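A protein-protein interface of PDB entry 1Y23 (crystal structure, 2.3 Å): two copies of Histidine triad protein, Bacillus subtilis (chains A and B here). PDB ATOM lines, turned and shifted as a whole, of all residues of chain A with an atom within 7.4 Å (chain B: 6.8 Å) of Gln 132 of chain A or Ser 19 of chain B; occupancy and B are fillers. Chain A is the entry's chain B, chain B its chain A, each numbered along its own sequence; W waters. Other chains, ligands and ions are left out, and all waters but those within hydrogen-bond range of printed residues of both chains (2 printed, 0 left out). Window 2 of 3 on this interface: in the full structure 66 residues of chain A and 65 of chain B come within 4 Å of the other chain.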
ATOM      1  N   LYS A 127      16.295   4.803  -3.323  1.00  0.00           N
ATOM      2  CA  LYS A 127      16.041   3.368  -3.378  1.00  0.00           C
ATOM      3  C   LYS A 127      14.579   3.126  -2.999  1.00  0.00           C
ATOM      4  O   LYS A 127      13.953   3.959  -2.341  1.00  0.00           O
ATOM      5  CB  LYS A 127      16.944   2.605  -2.398  1.00  0.00           C
ATOM      6  CG  LYS A 127      18.390   2.453  -2.842  1.00  0.00           C
ATOM      7  CD  LYS A 127      19.110   1.376  -2.030  1.00  0.00           C
ATOM      8  CE  LYS A 127      19.044   1.661  -0.532  1.00  0.00           C
ATOM      9  NZ  LYS A 127      19.659   2.988  -0.204  1.00  0.00           N
ATOM     10  N   PRO A 128      14.021   1.975  -3.399  1.00  0.00           N
ATOM     11  CA  PRO A 128      12.623   1.665  -3.081  1.00  0.00           C
ATOM     12  C   PRO A 128      12.259   1.819  -1.611  1.00  0.00           C
ATOM     13  O   PRO A 128      11.145   2.232  -1.282  1.00  0.00           O
ATOM     14  CB  PRO A 128      12.461   0.227  -3.578  1.00  0.00           C
ATOM     15  CG  PRO A 128      13.852  -0.328  -3.468  1.00  0.00           C
ATOM     16  CD  PRO A 128      14.683   0.815  -4.017  1.00  0.00           C
ATOM     17  N   GLU A 129      13.189   1.503  -0.719  1.00  0.00           N
ATOM     18  CA  GLU A 129      12.882   1.621   0.698  1.00  0.00           C
ATOM     19  C   GLU A 129      12.881   3.061   1.190  1.00  0.00           C
ATOM     20  O   GLU A 129      12.165   3.387   2.136  1.00  0.00           O
ATOM     21  CB  GLU A 129      13.851   0.801   1.540  1.00  0.00           C
ATOM     22  CG  GLU A 129      13.144  -0.219   2.410  1.00  0.00           C
ATOM     23  CD  GLU A 129      14.004  -0.687   3.561  1.00  0.00           C
ATOM     24  OE1 GLU A 129      15.202  -0.987   3.323  1.00  0.00           O
ATOM     25  OE2 GLU A 129      13.483  -0.764   4.701  1.00  0.00           O
ATOM     26  N   ASP A 130      13.681   3.917   0.564  1.00  0.00           N
ATOM     27  CA  ASP A 130      13.725   5.318   0.967  1.00  0.00           C
ATOM     28  C   ASP A 130      12.376   5.953   0.625  1.00  0.00           C
ATOM     29  O   ASP A 130      11.765   6.641   1.450  1.00  0.00           O
ATOM     30  CB  ASP A 130      14.848   6.065   0.237  1.00  0.00           C
ATOM     31  CG  ASP A 130      16.203   5.407   0.411  1.00  0.00           C
ATOM     32  OD1 ASP A 130      16.586   5.096   1.565  1.00  0.00           O
ATOM     33  OD2 ASP A 130      16.895   5.208  -0.612  1.00  0.00           O
ATOM     34  N   LEU A 131      11.926   5.708  -0.601  1.00  0.00           N
ATOM     35  CA  LEU A 131      10.653   6.227  -1.088  1.00  0.00           C
ATOM     36  C   LEU A 131       9.518   5.804  -0.163  1.00  0.00           C
ATOM     37  O   LEU A 131       8.624   6.594   0.147  1.00  0.00           O
ATOM     38  CB  LEU A 131      10.395   5.712  -2.511  1.00  0.00           C
ATOM     39  CG  LEU A 131      10.703   6.642  -3.689  1.00  0.00           C
ATOM     40  CD1 LEU A 131      11.912   7.522  -3.402  1.00  0.00           C
ATOM     41  CD2 LEU A 131      10.919   5.804  -4.941  1.00  0.00           C
ATOM     42  N   GLN A 132       9.578   4.556   0.289  1.00  0.00           N
ATOM     43  CA  GLN A 132       8.566   3.990   1.172  1.00  0.00           C
ATOM     44  C   GLN A 132       8.578   4.663   2.552  1.00  0.00           C
ATOM     45  O   GLN A 132       7.528   4.828   3.183  1.00  0.00           O
ATOM     46  CB  GLN A 132       8.803   2.482   1.310  1.00  0.00           C
ATOM     47  CG  GLN A 132       7.533   1.639   1.319  1.00  0.00           C
ATOM     48  CD  GLN A 132       6.555   2.039   0.219  1.00  0.00           C
ATOM     49  OE1 GLN A 132       5.818   3.015   0.366  1.00  0.00           O
ATOM     50  NE2 GLN A 132       6.556   1.299  -0.892  1.00  0.00           N
ATOM     51  N   ASN A 133       9.768   5.041   3.016  1.00  0.00           N
ATOM     52  CA  ASN A 133       9.908   5.707   4.308  1.00  0.00           C
ATOM     53  C   ASN A 133       9.413   7.145   4.195  1.00  0.00           C
ATOM     54  O   ASN A 133       8.740   7.659   5.095  1.00  0.00           O
ATOM     55  CB  ASN A 133      11.372   5.700   4.776  1.00  0.00           C
ATOM     56  CG  ASN A 133      11.869   4.305   5.127  1.00  0.00           C
ATOM     57  OD1 ASN A 133      11.100   3.456   5.585  1.00  0.00           O
ATOM     58  ND2 ASN A 133      13.161   4.069   4.932  1.00  0.00           N
ATOM     59  N   ILE A 134       9.754   7.784   3.077  1.00  0.00           N
ATOM     60  CA  ILE A 134       9.339   9.160   2.811  1.00  0.00           C
ATOM     61  C   ILE A 134       7.813   9.240   2.717  1.00  0.00           C
ATOM     62  O   ILE A 134       7.174  10.011   3.442  1.00  0.00           O
ATOM     63  CB  ILE A 134       9.948   9.685   1.495  1.00  0.00           C
ATOM     64  CG1 ILE A 134      11.481   9.750   1.627  1.00  0.00           C
ATOM     65  CG2 ILE A 134       9.362  11.062   1.155  1.00  0.00           C
ATOM     66  CD1 ILE A 134      12.201  10.155   0.340  1.00  0.00           C
ATOM     67  N   SER A 135       7.231   8.438   1.835  1.00  0.00           N
ATOM     68  CA  SER A 135       5.789   8.444   1.666  1.00  0.00           C
ATOM     69  C   SER A 135       5.103   8.075   2.969  1.00  0.00           C
ATOM     70  O   SER A 135       4.093   8.673   3.349  1.00  0.00           O
ATOM     71  CB  SER A 135       5.364   7.464   0.565  1.00  0.00           C
ATOM     72  OG  SER A 135       5.611   6.116   0.929  1.00  0.00           O
ATOM     73  N   SER A 136       5.655   7.089   3.663  1.00  0.00           N
ATOM     74  CA  SER A 136       5.072   6.648   4.922  1.00  0.00           C
ATOM     75  C   SER A 136       5.024   7.780   5.945  1.00  0.00           C
ATOM     76  O   SER A 136       4.096   7.860   6.750  1.00  0.00           O
ATOM     77  CB  SER A 136       5.864   5.461   5.482  1.00  0.00           C
ATOM     78  OG  SER A 136       5.219   4.927   6.622  1.00  0.00           O
ATOM     79  N   SER A 137       6.021   8.657   5.911  1.00  0.00           N
ATOM     80  CA  SER A 137       6.072   9.784   6.840  1.00  0.00           C
ATOM     81  C   SER A 137       5.020  10.831   6.515  1.00  0.00           C
ATOM     82  O   SER A 137       4.373  11.365   7.411  1.00  0.00           O
ATOM     83  CB  SER A 137       7.441  10.456   6.797  1.00  0.00           C
ATOM     84  OG  SER A 137       8.464   9.538   7.122  1.00  0.00           O
ATOM     85  N   ILE A 138       4.866  11.140   5.230  1.00  0.00           N
ATOM     86  CA  ILE A 138       3.890  12.142   4.830  1.00  0.00           C
ATOM     87  C   ILE A 138       2.507  11.622   5.126  1.00  0.00           C
ATOM     88  O   ILE A 138       1.653  12.346   5.621  1.00  0.00           O
ATOM     89  CB  ILE A 138       3.954  12.448   3.335  1.00  0.00           C
ATOM     90  CG1 ILE A 138       5.373  12.859   2.942  1.00  0.00           C
ATOM     91  CG2 ILE A 138       2.973  13.561   3.002  1.00  0.00           C
ATOM     92  CD1 ILE A 138       5.544  13.067   1.450  1.00  0.00           C
ATOM     93  N   ILE B  12      -1.657   1.397 -11.026  1.00  0.00           N
ATOM     94  CA  ILE B  12      -1.135   1.703  -9.697  1.00  0.00           C
ATOM     95  C   ILE B  12      -2.319   1.746  -8.735  1.00  0.00           C
ATOM     96  O   ILE B  12      -2.234   1.266  -7.608  1.00  0.00           O
ATOM     97  CB  ILE B  12      -0.424   3.085  -9.687  1.00  0.00           C
ATOM     98  CG1 ILE B  12       0.883   3.005 -10.484  1.00  0.00           C
ATOM     99  CG2 ILE B  12      -0.179   3.542  -8.254  1.00  0.00           C
ATOM    100  CD1 ILE B  12       1.701   4.270 -10.472  1.00  0.00           C
ATOM    101  N   ILE B  13      -3.416   2.332  -9.206  1.00  0.00           N
ATOM    102  CA  ILE B  13      -4.645   2.468  -8.437  1.00  0.00           C
ATOM    103  C   ILE B  13      -5.204   1.085  -8.130  1.00  0.00           C
ATOM    104  O   ILE B  13      -5.614   0.803  -7.010  1.00  0.00           O
ATOM    105  CB  ILE B  13      -5.696   3.284  -9.241  1.00  0.00           C
ATOM    106  CG1 ILE B  13      -5.196   4.712  -9.453  1.00  0.00           C
ATOM    107  CG2 ILE B  13      -7.032   3.311  -8.516  1.00  0.00           C
ATOM    108  CD1 ILE B  13      -5.971   5.478 -10.486  1.00  0.00           C
ATOM    109  N   ILE B  17       0.775  -2.333 -10.108  1.00  0.00           N
ATOM    110  CA  ILE B  17       2.115  -1.764 -10.010  1.00  0.00           C
ATOM    111  C   ILE B  17       2.275  -1.186  -8.605  1.00  0.00           C
ATOM    112  O   ILE B  17       1.395  -0.472  -8.119  1.00  0.00           O
ATOM    113  CB  ILE B  17       2.314  -0.608 -11.012  1.00  0.00           C
ATOM    114  CG1 ILE B  17       2.050  -1.092 -12.428  1.00  0.00           C
ATOM    115  CG2 ILE B  17       3.718  -0.045 -10.879  1.00  0.00           C
ATOM    116  CD1 ILE B  17       2.083   0.019 -13.456  1.00  0.00           C
ATOM    117  N   PRO B  18       3.395  -1.487  -7.932  1.00  0.00           N
ATOM    118  CA  PRO B  18       3.618  -0.962  -6.580  1.00  0.00           C
ATOM    119  C   PRO B  18       3.840   0.554  -6.599  1.00  0.00           C
ATOM    120  O   PRO B  18       4.152   1.124  -7.643  1.00  0.00           O
ATOM    121  CB  PRO B  18       4.852  -1.729  -6.119  1.00  0.00           C
ATOM    122  CG  PRO B  18       5.611  -1.929  -7.399  1.00  0.00           C
ATOM    123  CD  PRO B  18       4.517  -2.342  -8.360  1.00  0.00           C
ATOM    124  N   SER B  19       3.671   1.199  -5.449  1.00  0.00           N
ATOM    125  CA  SER B  19       3.862   2.642  -5.345  1.00  0.00           C
ATOM    126  C   SER B  19       4.076   3.072  -3.898  1.00  0.00           C
ATOM    127  O   SER B  19       3.643   2.391  -2.973  1.00  0.00           O
ATOM    128  CB  SER B  19       2.646   3.389  -5.918  1.00  0.00           C
ATOM    129  OG  SER B  19       1.474   3.141  -5.146  1.00  0.00           O
ATOM    130  N   ALA B  20       4.756   4.198  -3.705  1.00  0.00           N
ATOM    131  CA  ALA B  20       4.998   4.715  -2.367  1.00  0.00           C
ATOM    132  C   ALA B  20       3.813   5.618  -2.043  1.00  0.00           C
ATOM    133  O   ALA B  20       3.862   6.832  -2.262  1.00  0.00           O
ATOM    134  CB  ALA B  20       6.297   5.503  -2.337  1.00  0.00           C
ATOM    135  N   LYS B  21       2.747   5.004  -1.530  1.00  0.00           N
ATOM    136  CA  LYS B  21       1.515   5.718  -1.202  1.00  0.00           C
ATOM    137  C   LYS B  21       1.638   6.789  -0.124  1.00  0.00           C
ATOM    138  O   LYS B  21       2.119   6.548   0.985  1.00  0.00           O
ATOM    139  CB  LYS B  21       0.402   4.725  -0.826  1.00  0.00           C
ATOM    140  CG  LYS B  21      -0.147   3.953  -2.022  1.00  0.00           C
ATOM    141  CD  LYS B  21      -1.312   3.051  -1.644  1.00  0.00           C
ATOM    142  CE  LYS B  21      -1.859   2.285  -2.855  1.00  0.00           C
ATOM    143  NZ  LYS B  21      -3.049   1.443  -2.484  1.00  0.00           N
ATOM    144  N   VAL B  22       1.185   7.984  -0.477  1.00  0.00           N
ATOM    145  CA  VAL B  22       1.220   9.120   0.428  1.00  0.00           C
ATOM    146  C   VAL B  22      -0.177   9.415   0.979  1.00  0.00           C
ATOM    147  O   VAL B  22      -0.345   9.803   2.140  1.00  0.00           O
ATOM    148  CB  VAL B  22       1.741  10.365  -0.315  1.00  0.00           C
ATOM    149  CG1 VAL B  22       1.629  11.602   0.557  1.00  0.00           C
ATOM    150  CG2 VAL B  22       3.179  10.141  -0.731  1.00  0.00           C
ATOM    151  N   LEU B  29      -5.918   9.033  -4.938  1.00  0.00           N
ATOM    152  CA  LEU B  29      -4.707   8.309  -4.588  1.00  0.00           C
ATOM    153  C   LEU B  29      -3.521   9.229  -4.888  1.00  0.00           C
ATOM    154  O   LEU B  29      -3.430   9.816  -5.981  1.00  0.00           O
ATOM    155  CB  LEU B  29      -4.568   7.008  -5.401  1.00  0.00           C
ATOM    156  CG  LEU B  29      -3.312   6.180  -5.058  1.00  0.00           C
ATOM    157  CD1 LEU B  29      -3.440   5.668  -3.614  1.00  0.00           C
ATOM    158  CD2 LEU B  29      -3.137   4.999  -6.014  1.00  0.00           C
ATOM    159  N   ALA B  30      -2.632   9.381  -3.908  1.00  0.00           N
ATOM    160  CA  ALA B  30      -1.432  10.202  -4.076  1.00  0.00           C
ATOM    161  C   ALA B  30      -0.236   9.338  -3.717  1.00  0.00           C
ATOM    162  O   ALA B  30      -0.277   8.584  -2.749  1.00  0.00           O
ATOM    163  CB  ALA B  30      -1.478  11.437  -3.171  1.00  0.00           C
ATOM    164  N   PHE B  31       0.821   9.450  -4.508  1.00  0.00           N
ATOM    165  CA  PHE B  31       2.032   8.679  -4.298  1.00  0.00           C
ATOM    166  C   PHE B  31       3.240   9.477  -4.802  1.00  0.00           C
ATOM    167  O   PHE B  31       3.100  10.419  -5.596  1.00  0.00           O
ATOM    168  CB  PHE B  31       1.914   7.319  -5.016  1.00  0.00           C
ATOM    169  CG  PHE B  31       1.433   7.420  -6.443  1.00  0.00           C
ATOM    170  CD1 PHE B  31       2.328   7.649  -7.482  1.00  0.00           C
ATOM    171  CD2 PHE B  31       0.078   7.303  -6.745  1.00  0.00           C
ATOM    172  CE1 PHE B  31       1.883   7.760  -8.803  1.00  0.00           C
ATOM    173  CE2 PHE B  31      -0.376   7.416  -8.063  1.00  0.00           C
ATOM    174  CZ  PHE B  31       0.527   7.644  -9.093  1.00  0.00           C
ATOM    175  N   LEU B  32       4.424   9.115  -4.322  1.00  0.00           N
ATOM    176  CA  LEU B  32       5.634   9.814  -4.722  1.00  0.00           C
ATOM    177  C   LEU B  32       5.956   9.596  -6.191  1.00  0.00           C
ATOM    178  O   LEU B  32       5.668   8.545  -6.756  1.00  0.00           O
ATOM    179  CB  LEU B  32       6.817   9.355  -3.868  1.00  0.00           C
ATOM    180  CG  LEU B  32       6.664   9.684  -2.380  1.00  0.00           C
ATOM    181  CD1 LEU B  32       7.742   8.980  -1.564  1.00  0.00           C
ATOM    182  CD2 LEU B  32       6.735  11.192  -2.198  1.00  0.00           C
HETATM  183  O   HOH W   1       3.173   2.582   0.088  1.00  0.00           O
HETATM  184  O   HOH W   2       3.395   4.152   2.715  1.00  0.00           O
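N of Leu 32 of chain B sits at hydrogen-bond distance from O of Ala 20 of chain B. The backbone carbonyl oxygen (O) of Ala 30 of chain B lies within hydrogen-bond range of the backbone NH (N) of Val 22 of chain B, 2.8 Å away. O of Leu 131 of chain A sits at hydrogen-bond distance from OG of Ser 135 of chain A (3.1 Å). The side-chain amide oxygen (OE1) of Gln 132 of chain A lies within hydrogen-bond range of the side-chain hydroxyl (OG) of Ser 135 of chain A (3.2 Å).
Among the printed residues, pairs that only touch across the chains: Leu 131 of chain A with Ala 20 of chain B, Leu 131 of chain A with Leu 32 of chain B, Gln 132 of chain A with Ser 19 of chain B, Gln 132 of chain A with Ala 20 of chain B, Ile 134 of chain A with Leu 32 of chain B, Ser 135 of chain A with Ala 20 of chain B, Ser 135 of chain A with Lys 21 of chain B, Ser 135 of chain A with Val 22 of chain B, Ser 135 of chain A with Leu 32 of chain B and Ile 138 of chain A with Val 22 of chain B.
Gln 132 of chain A touches two residues of chain B. Ser 19 of chain B touches one residue of chain A. Printed residues of chain A within 4 Å of Lys 21 of chain B: Ser 135. Printed residues of chain B within 4 Å of Ile 134 of chain A: Leu 32 (3.8 Å). Phe 31 of chain B touches none of the printed residues of chain A. Ile 13 of chain B touches none of the printed residues of chain A. The nearest residue of chain B that does not touch Gln 132 of chain A is Lys 21 of chain B (4.1 Å). The nearest printed residue of chain B that does not touch Leu 131 of chain A is Lys 21 of chain B (6.3 Å).
Of the 12 printed residues of chain A, 5 touch a printed residue of chain B. Hydrophobic or aromatic side chains of chain A within 4 Å of the printed part of chain B: Ile 134 and Ile 138. Of the 12 printed residues of chain B, 5 touch a printed residue of chain A. Hydrophobic or aromatic side chains of chain B that line the printed part of chain A: Ala 20, Val 22 and Leu 32. Among the printed residues, 10 pairs touch across the chains.
No position is printed for both chains. Of the 10 pairs that touch across the chains among the printed residues, none has its exchanged pair printed and touching as well.
Water W1 lies within hydrogen-bond range of the side-chain amide oxygen of Gln 132 of chain A (2.7 Å), the backbone NH of Lys 21 of chain B (2.9 Å) and the backbone carbonyl oxygen of Ser 19 of chain B (3.1 Å). Water W2 lies within hydrogen-bond range of O of Lys 21 of chain B (3.2 Å) and OG of Ser 135 of chain A (3.5 Å).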
